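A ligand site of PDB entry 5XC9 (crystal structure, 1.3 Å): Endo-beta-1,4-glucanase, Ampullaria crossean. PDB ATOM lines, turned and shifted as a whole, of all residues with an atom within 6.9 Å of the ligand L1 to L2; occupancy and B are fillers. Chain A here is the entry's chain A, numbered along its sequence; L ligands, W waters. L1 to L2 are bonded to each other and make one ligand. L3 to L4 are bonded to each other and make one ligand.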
ATOM      1  N   THR A  27      16.634  19.440  13.334  1.00  0.00           N
ATOM      2  CA  THR A  27      16.848  18.622  14.515  1.00  0.00           C
ATOM      3  C   THR A  27      15.795  18.943  15.556  1.00  0.00           C
ATOM      4  O   THR A  27      15.235  20.055  15.590  1.00  0.00           O
ATOM      5  CB  THR A  27      18.221  18.789  15.134  1.00  0.00           C
ATOM      6  OG1 THR A  27      18.365  20.078  15.774  1.00  0.00           O
ATOM      7  CG2 THR A  27      19.329  18.582  14.151  1.00  0.00           C
ATOM      8  N   THR A  28      15.492  17.951  16.408  1.00  0.00           N
ATOM      9  CA  THR A  28      14.692  18.111  17.619  1.00  0.00           C
ATOM     10  C   THR A  28      15.356  17.297  18.703  1.00  0.00           C
ATOM     11  O   THR A  28      16.390  16.676  18.483  1.00  0.00           O
ATOM     12  CB  THR A  28      13.243  17.659  17.390  1.00  0.00           C
ATOM     13  OG1 THR A  28      13.227  16.349  16.772  1.00  0.00           O
ATOM     14  CG2 THR A  28      12.423  18.625  16.520  1.00  0.00           C
ATOM     15  N   ARG A  29      14.766  17.279  19.890  1.00  0.00           N
ATOM     16  CA  ARG A  29      15.238  16.452  20.990  1.00  0.00           C
ATOM     17  C   ARG A  29      14.078  15.613  21.499  1.00  0.00           C
ATOM     18  O   ARG A  29      12.916  16.046  21.432  1.00  0.00           O
ATOM     19  CB  ARG A  29      15.859  17.286  22.114  1.00  0.00           C
ATOM     20  CG  ARG A  29      14.977  18.349  22.628  1.00  0.00           C
ATOM     21  CD  ARG A  29      15.763  19.342  23.531  1.00  0.00           C
ATOM     22  NE  ARG A  29      14.912  20.398  24.045  1.00  0.00           N
ATOM     23  CZ  ARG A  29      14.499  21.500  23.378  1.00  0.00           C
ATOM     24  NH1 ARG A  29      14.823  21.736  22.096  1.00  0.00           N
ATOM     25  NH2 ARG A  29      13.738  22.359  24.019  1.00  0.00           N
ATOM     26  N   TYR A  30      14.399  14.446  22.036  1.00  0.00           N
ATOM     27  CA  TYR A  30      13.373  13.571  22.550  1.00  0.00           C
ATOM     28  C   TYR A  30      13.840  12.852  23.802  1.00  0.00           C
ATOM     29  O   TYR A  30      15.039  12.654  24.024  1.00  0.00           O
ATOM     30  CB  TYR A  30      12.915  12.533  21.515  1.00  0.00           C
ATOM     31  CG  TYR A  30      13.790  11.325  21.287  1.00  0.00           C
ATOM     32  CD1 TYR A  30      14.943  11.403  20.493  1.00  0.00           C
ATOM     33  CD2 TYR A  30      13.430  10.117  21.806  1.00  0.00           C
ATOM     34  CE1 TYR A  30      15.709  10.274  20.239  1.00  0.00           C
ATOM     35  CE2 TYR A  30      14.169   8.980  21.565  1.00  0.00           C
ATOM     36  CZ  TYR A  30      15.321   9.073  20.771  1.00  0.00           C
ATOM     37  OH  TYR A  30      16.019   7.901  20.533  1.00  0.00           O
ATOM     38  N   VAL A  31      12.855  12.391  24.577  1.00  0.00           N
ATOM     39  CA  VAL A  31      13.053  11.587  25.776  1.00  0.00           C
ATOM     40  C   VAL A  31      11.889  10.586  25.823  1.00  0.00           C
ATOM     41  O   VAL A  31      10.737  11.001  25.936  1.00  0.00           O
ATOM     42  CB  VAL A  31      13.061  12.460  27.047  1.00  0.00           C
ATOM     43  CG1 VAL A  31      13.246  11.585  28.235  1.00  0.00           C
ATOM     44  CG2 VAL A  31      14.094  13.624  27.005  1.00  0.00           C
ATOM     45  N   ASP A  32      12.172   9.269  25.747  1.00  0.00           N
ATOM     46  CA  ASP A  32      11.069   8.298  25.881  1.00  0.00           C
ATOM     47  C   ASP A  32      11.435   7.013  26.620  1.00  0.00           C
ATOM     48  O   ASP A  32      10.529   6.241  26.938  1.00  0.00           O
ATOM     49  CB  ASP A  32      10.352   7.991  24.548  1.00  0.00           C
ATOM     50  CG  ASP A  32      11.225   7.233  23.538  1.00  0.00           C
ATOM     51  OD1 ASP A  32      12.233   6.641  23.925  1.00  0.00           O
ATOM     52  OD2 ASP A  32      10.851   7.182  22.355  1.00  0.00           O
ATOM     53  N   GLY A  93      10.047  30.250  16.025  1.00  0.00           N
ATOM     54  CA  GLY A  93       9.060  29.741  16.925  1.00  0.00           C
ATOM     55  C   GLY A  93       9.308  28.325  17.373  1.00  0.00           C
ATOM     56  O   GLY A  93       8.619  27.844  18.277  1.00  0.00           O
ATOM     57  N   LYS A  94      10.287  27.636  16.781  1.00  0.00           N
ATOM     58  CA  LYS A  94      10.503  26.225  17.040  1.00  0.00           C
ATOM     59  C   LYS A  94      11.969  25.934  17.224  1.00  0.00           C
ATOM     60  O   LYS A  94      12.465  24.880  16.820  1.00  0.00           O
ATOM     61  CB  LYS A  94       9.905  25.348  15.927  1.00  0.00           C
ATOM     62  CG  LYS A  94       8.356  25.458  15.924  1.00  0.00           C
ATOM     63  CD  LYS A  94       7.706  24.779  14.761  1.00  0.00           C
ATOM     64  CE  LYS A  94       6.185  24.736  14.971  1.00  0.00           C
ATOM     65  NZ  LYS A  94       5.436  24.410  13.769  1.00  0.00           N
ATOM     66  N   GLY A  95      12.697  26.859  17.829  1.00  0.00           N
ATOM     67  CA  GLY A  95      14.103  26.662  18.105  1.00  0.00           C
ATOM     68  C   GLY A  95      14.779  27.993  18.383  1.00  0.00           C
ATOM     69  O   GLY A  95      14.136  29.022  18.509  1.00  0.00           O
ATOM     70  N   CYS A 112      12.708   7.797  13.899  1.00  0.00           N
ATOM     71  CA  CYS A 112      11.607   8.756  14.044  1.00  0.00           C
ATOM     72  C   CYS A 112      10.586   8.446  12.947  1.00  0.00           C
ATOM     73  O   CYS A 112      10.809   8.783  11.760  1.00  0.00           O
ATOM     74  CB  CYS A 112      12.144  10.167  13.888  1.00  0.00           C
ATOM     75  SG  CYS A 112      10.836  11.439  14.105  1.00  0.00           S
ATOM     76  N   PRO A 113       9.495   7.732  13.264  1.00  0.00           N
ATOM     77  CA  PRO A 113       8.557   7.296  12.222  1.00  0.00           C
ATOM     78  C   PRO A 113       7.752   8.450  11.680  1.00  0.00           C
ATOM     79  O   PRO A 113       7.485   9.429  12.373  1.00  0.00           O
ATOM     80  CB  PRO A 113       7.634   6.304  12.968  1.00  0.00           C
ATOM     81  CG  PRO A 113       7.736   6.734  14.390  1.00  0.00           C
ATOM     82  CD  PRO A 113       9.094   7.292  14.616  1.00  0.00           C
ATOM     83  N   GLY A 116       2.794   9.922  13.468  1.00  0.00           N
ATOM     84  CA  GLY A 116       2.907  10.660  14.709  1.00  0.00           C
ATOM     85  C   GLY A 116       3.953  11.740  14.725  1.00  0.00           C
ATOM     86  O   GLY A 116       4.042  12.475  15.725  1.00  0.00           O
ATOM     87  N   ASN A 117       4.749  11.865  13.670  1.00  0.00           N
ATOM     88  CA  ASN A 117       5.806  12.880  13.604  1.00  0.00           C
ATOM     89  C   ASN A 117       5.812  13.519  12.223  1.00  0.00           C
ATOM     90  O   ASN A 117       6.861  13.677  11.604  1.00  0.00           O
ATOM     91  CB  ASN A 117       7.180  12.265  13.886  1.00  0.00           C
ATOM     92  CG  ASN A 117       7.241  11.647  15.244  1.00  0.00           C
ATOM     93  OD1 ASN A 117       7.362  12.340  16.251  1.00  0.00           O
ATOM     94  ND2 ASN A 117       7.169  10.318  15.277  1.00  0.00           N
ATOM     95  N   GLU A 118       4.648  13.911  11.744  1.00  0.00           N
ATOM     96  CA  GLU A 118       4.558  14.288  10.352  1.00  0.00           C
ATOM     97  C   GLU A 118       5.332  15.569  10.072  1.00  0.00           C
ATOM     98  O   GLU A 118       6.022  15.660   9.049  1.00  0.00           O
ATOM     99  CB  GLU A 118       3.078  14.386   9.979  1.00  0.00           C
ATOM    100  CG  GLU A 118       2.356  12.966   9.996  1.00  0.00           C
ATOM    101  CD  GLU A 118       1.808  12.499  11.382  1.00  0.00           C
ATOM    102  OE1 GLU A 118       1.140  11.398  11.448  1.00  0.00           O
ATOM    103  OE2 GLU A 118       2.033  13.205  12.395  1.00  0.00           O
ATOM    104  N   GLU A 119       5.287  16.551  10.976  1.00  0.00           N
ATOM    105  CA  GLU A 119       5.901  17.854  10.709  1.00  0.00           C
ATOM    106  C   GLU A 119       7.399  17.726  10.448  1.00  0.00           C
ATOM    107  O   GLU A 119       7.936  18.320   9.505  1.00  0.00           O
ATOM    108  CB  GLU A 119       5.692  18.769  11.928  1.00  0.00           C
ATOM    109  CG  GLU A 119       6.475  20.075  11.869  1.00  0.00           C
ATOM    110  CD  GLU A 119       6.172  21.038  12.985  1.00  0.00           C
ATOM    111  OE1 GLU A 119       6.665  22.167  12.872  1.00  0.00           O
ATOM    112  OE2 GLU A 119       5.436  20.679  13.948  1.00  0.00           O
ATOM    113  N   TRP A 120       8.099  16.972  11.285  1.00  0.00           N
ATOM    114  CA  TRP A 120       9.543  16.897  11.188  1.00  0.00           C
ATOM    115  C   TRP A 120      10.039  15.655  10.467  1.00  0.00           C
ATOM    116  O   TRP A 120      11.006  15.720   9.715  1.00  0.00           O
ATOM    117  CB  TRP A 120      10.170  16.872  12.583  1.00  0.00           C
ATOM    118  CG  TRP A 120       9.919  18.135  13.385  1.00  0.00           C
ATOM    119  CD1 TRP A 120       9.044  18.258  14.447  1.00  0.00           C
ATOM    120  CD2 TRP A 120      10.525  19.440  13.222  1.00  0.00           C
ATOM    121  NE1 TRP A 120       9.070  19.552  14.931  1.00  0.00           N
ATOM    122  CE2 TRP A 120       9.964  20.282  14.202  1.00  0.00           C
ATOM    123  CE3 TRP A 120      11.477  19.963  12.345  1.00  0.00           C
ATOM    124  CZ2 TRP A 120      10.344  21.606  14.352  1.00  0.00           C
ATOM    125  CZ3 TRP A 120      11.849  21.279  12.503  1.00  0.00           C
ATOM    126  CH2 TRP A 120      11.291  22.079  13.498  1.00  0.00           C
ATOM    127  N   CYS A 121       9.402  14.500  10.715  1.00  0.00           N
ATOM    128  CA  CYS A 121       9.894  13.226  10.162  1.00  0.00           C
ATOM    129  C   CYS A 121       9.096  12.745   8.973  1.00  0.00           C
ATOM    130  O   CYS A 121       9.450  11.696   8.391  1.00  0.00           O
ATOM    131  CB  CYS A 121       9.934  12.159  11.262  1.00  0.00           C
ATOM    132  SG  CYS A 121      11.054  12.718  12.559  1.00  0.00           S
ATOM    133  N   HIS A 140      15.731  14.559   8.919  1.00  0.00           N
ATOM    134  CA  HIS A 140      15.545  15.101  10.245  1.00  0.00           C
ATOM    135  C   HIS A 140      16.250  14.194  11.242  1.00  0.00           C
ATOM    136  O   HIS A 140      16.163  12.976  11.119  1.00  0.00           O
ATOM    137  CB  HIS A 140      14.044  15.138  10.588  1.00  0.00           C
ATOM    138  CG  HIS A 140      13.790  15.793  11.885  1.00  0.00           C
ATOM    139  ND1 HIS A 140      13.821  17.167  12.034  1.00  0.00           N
ATOM    140  CD2 HIS A 140      13.607  15.266  13.117  1.00  0.00           C
ATOM    141  CE1 HIS A 140      13.643  17.460  13.311  1.00  0.00           C
ATOM    142  NE2 HIS A 140      13.525  16.324  13.992  1.00  0.00           N
ATOM    143  N   ASP A 142      16.274  13.393  15.273  1.00  0.00           N
ATOM    144  CA  ASP A 142      15.730  13.569  16.614  1.00  0.00           C
ATOM    145  C   ASP A 142      16.832  13.127  17.587  1.00  0.00           C
ATOM    146  O   ASP A 142      17.354  12.014  17.475  1.00  0.00           O
ATOM    147  CB  ASP A 142      14.467  12.732  16.762  1.00  0.00           C
ATOM    148  CG  ASP A 142      13.516  13.230  17.843  1.00  0.00           C
ATOM    149  OD1 ASP A 142      13.700  14.327  18.396  1.00  0.00           O
ATOM    150  OD2 ASP A 142      12.557  12.466  18.109  1.00  0.00           O
ATOM    151  N   ASP A 156      18.822  24.127  20.817  1.00  0.00           N
ATOM    152  CA  ASP A 156      17.352  24.202  20.804  1.00  0.00           C
ATOM    153  C   ASP A 156      16.917  24.070  19.353  1.00  0.00           C
ATOM    154  O   ASP A 156      16.769  25.050  18.634  1.00  0.00           O
ATOM    155  CB  ASP A 156      16.881  25.499  21.446  1.00  0.00           C
ATOM    156  CG  ASP A 156      15.372  25.603  21.528  1.00  0.00           C
ATOM    157  OD1 ASP A 156      14.685  24.590  21.285  1.00  0.00           O
ATOM    158  OD2 ASP A 156      14.879  26.725  21.815  1.00  0.00           O
ATOM    159  N   ASN A 157      16.778  22.819  18.908  1.00  0.00           N
ATOM    160  CA  ASN A 157      16.373  22.497  17.547  1.00  0.00           C
ATOM    161  C   ASN A 157      17.168  23.252  16.477  1.00  0.00           C
ATOM    162  O   ASN A 157      16.587  23.785  15.536  1.00  0.00           O
ATOM    163  CB  ASN A 157      14.890  22.760  17.338  1.00  0.00           C
ATOM    164  CG  ASN A 157      13.990  22.012  18.308  1.00  0.00           C
ATOM    165  OD1 ASN A 157      14.370  21.094  19.009  1.00  0.00           O
ATOM    166  ND2 ASN A 157      12.748  22.439  18.340  1.00  0.00           N
HETATM  167  C1  LIG L   1       8.894  21.469  18.559  1.00  0.00           C
HETATM  168  C2  LIG L   1       8.530  20.010  18.886  1.00  0.00           C
HETATM  169  C3  LIG L   1       9.728  19.251  19.435  1.00  0.00           C
HETATM  170  C4  LIG L   1      10.362  20.057  20.571  1.00  0.00           C
HETATM  171  C5  LIG L   1      11.648  19.496  21.140  1.00  0.00           C
HETATM  172  C6  LIG L   1       9.545  22.141  19.729  1.00  0.00           C
HETATM  173  O1  LIG L   1      10.026  23.429  19.377  1.00  0.00           O
HETATM  174  O2  LIG L   1       7.714  22.232  18.267  1.00  0.00           O
HETATM  175  O3  LIG L   1       8.031  19.401  17.703  1.00  0.00           O
HETATM  176  O4  LIG L   1       9.232  18.030  19.985  1.00  0.00           O
HETATM  177  O5  LIG L   1      10.667  21.351  20.078  1.00  0.00           O
HETATM  178  O6  LIG L   1      12.573  19.253  20.076  1.00  0.00           O
HETATM  179  C1  LG2 L   2       9.506  15.782  20.656  1.00  0.00           C
HETATM  180  C2  LG2 L   2       9.950  14.403  20.210  1.00  0.00           C
HETATM  181  C3  LG2 L   2       9.482  14.116  18.797  1.00  0.00           C
HETATM  182  C4  LG2 L   2      10.031  15.227  17.895  1.00  0.00           C
HETATM  183  C5  LG2 L   2       9.733  15.080  16.413  1.00  0.00           C
HETATM  184  C6  LG2 L   2       9.913  16.835  19.628  1.00  0.00           C
HETATM  185  O1  LG2 L   2      10.152  16.074  21.904  1.00  0.00           O
HETATM  186  O2  LG2 L   2       9.405  13.434  21.123  1.00  0.00           O
HETATM  187  O3  LG2 L   2       9.985  12.850  18.380  1.00  0.00           O
HETATM  188  O4  LG2 L   2       9.473  16.465  18.340  1.00  0.00           O
HETATM  189  O5  LG2 L   2       8.319  14.939  16.201  1.00  0.00           O
HETATM  190  C1  LG3 L   3      10.673   4.722  19.838  1.00  0.00           C
HETATM  191  C2  LG3 L   3      11.089   3.323  19.450  1.00  0.00           C
HETATM  192  C3  LG3 L   3      10.291   2.785  18.261  1.00  0.00           C
HETATM  193  C4  LG3 L   3      10.300   3.823  17.150  1.00  0.00           C
HETATM  194  C5  LG3 L   3       9.507   3.405  15.893  1.00  0.00           C
HETATM  195  C6  LG3 L   3      10.602   5.611  18.610  1.00  0.00           C
HETATM  196  O1  LG3 L   3      10.015   6.890  18.974  1.00  0.00           O
HETATM  197  O2  LG3 L   3      11.675   5.192  20.756  1.00  0.00           O
HETATM  198  O3  LG3 L   3      10.903   2.469  20.584  1.00  0.00           O
HETATM  199  O4  LG3 L   3      10.919   1.644  17.668  1.00  0.00           O
HETATM  200  O5  LG3 L   3       9.733   5.027  17.648  1.00  0.00           O
HETATM  201  O6  LG3 L   3       8.132   3.201  16.254  1.00  0.00           O
HETATM  202  C1  LG4 L   4      10.641  -0.654  17.138  1.00  0.00           C
HETATM  203  C2  LG4 L   4      10.199  -1.989  17.706  1.00  0.00           C
HETATM  204  C3  LG4 L   4      10.996  -2.306  18.957  1.00  0.00           C
HETATM  205  C4  LG4 L   4      10.955  -1.139  19.960  1.00  0.00           C
HETATM  206  C5  LG4 L   4      11.907  -1.352  21.123  1.00  0.00           C
HETATM  207  C6  LG4 L   4      10.492   0.401  18.210  1.00  0.00           C
HETATM  208  O1  LG4 L   4       9.796  -0.328  16.036  1.00  0.00           O
HETATM  209  O2  LG4 L   4      10.408  -3.035  16.759  1.00  0.00           O
HETATM  210  O3  LG4 L   4      10.496  -3.484  19.624  1.00  0.00           O
HETATM  211  O4  LG4 L   4      11.378   0.052  19.267  1.00  0.00           O
HETATM  212  O5  LG4 L   4      11.929  -0.160  21.908  1.00  0.00           O
HETATM  213  O   HOH W   1       6.544  16.852  17.677  1.00  0.00           O
HETATM  214  O   HOH W   2      10.030  10.229  20.616  1.00  0.00           O
HETATM  215  O   HOH W   3      11.955  24.545  21.148  1.00  0.00           O
HETATM  216  O   HOH W   4       6.922  15.844  13.883  1.00  0.00           O
HETATM  217  O   HOH W   5       8.144  10.809  18.769  1.00  0.00           O
HETATM  218  O   HOH W   6      10.175  13.598  23.948  1.00  0.00           O
HETATM  219  O   HOH W   7       8.602  17.994  23.423  1.00  0.00           O
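CB of Thr 28 touches O6 of LIG L1, 3.2 Å away.
Tyr 30 touches the ligand L1 to L2.
CA of Lys 94 touches O1 of LIG L1, at 3.7 Å.
Hydrophobic or aromatic side chains within 4 Å of the ligand L1 to L2: Tyr 30 and Trp 120.
OG1 of Thr 28 is in hydrogen-bond range of NE2 of His 140 (2.8 Å).
OD1 of Asp 142 is in hydrogen-bond range of OG1 of Thr 28 (2.6 Å).
The backbone NH of Arg 29 sits close to the side-chain carboxylate of Asp 142, 3.5 Å away.
The side-chain amide nitrogen of Asn 117 is in hydrogen-bond range of the backbone carbonyl oxygen of Pro 113, at 3.1 Å.
The guanidinium group (NH1) of Arg 29 is in salt-bridge range of the side-chain carboxylate (OD1) of Asp 156, at 3.0 Å.
The guanidinium group (NH1) of Arg 29 is in hydrogen-bond range of the side-chain amide oxygen (OD1) of Asn 157.
The side-chain sulfur (SG) of Cys 112 forms a disulfide with the side-chain sulfur (SG) of Cys 121, 2.0 Å away.
O of Lys 94 lies within hydrogen-bond range of ND2 of Asn 157 (2.9 Å).
An oxygen (O5) of LG2 L2 is in hydrogen-bond range of the side-chain amide oxygen of Asn 117 (2.8 Å).
O6 of LIG L1 sits at hydrogen-bond distance from N of Arg 29 (3.0 Å).
The side-chain carboxylate (OD2) of Asp 32 lies within hydrogen-bond range of an oxygen (O2) of LG3 L3, 2.7 Å away.
The backbone carbonyl oxygen of Arg 29 sits at hydrogen-bond distance from an oxygen (O1) of LG2 L2, 2.8 Å away.
O3 of LIG L1 lies within hydrogen-bond range of NE1 of Trp 120 (3.0 Å).
O3 of LG2 L2 is in hydrogen-bond range of OD2 of Asp 142.
The side-chain amide oxygen of Asn 157 is in hydrogen-bond range of an oxygen (O6) of LIG L1 (2.8 Å).
Water W5 bridges O3 of LG2 L2 (2.8 Å) and OD1 of Asn 117 (3.0 Å).
Water W3 lies within hydrogen-bond range of the side-chain carboxylate (OD1) of Asp 156 and an oxygen (O1) of LIG L1.
Water W4 lies within hydrogen-bond range of O5 of LG2 L2 (2.9 Å), N of Trp 120 (3.1 Å), O of Asn 117 (3.1 Å) and N of Glu 119 (3.4 Å).
Water W6 lies within hydrogen-bond range of O2 of LG2 L2 and N of Val 31.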
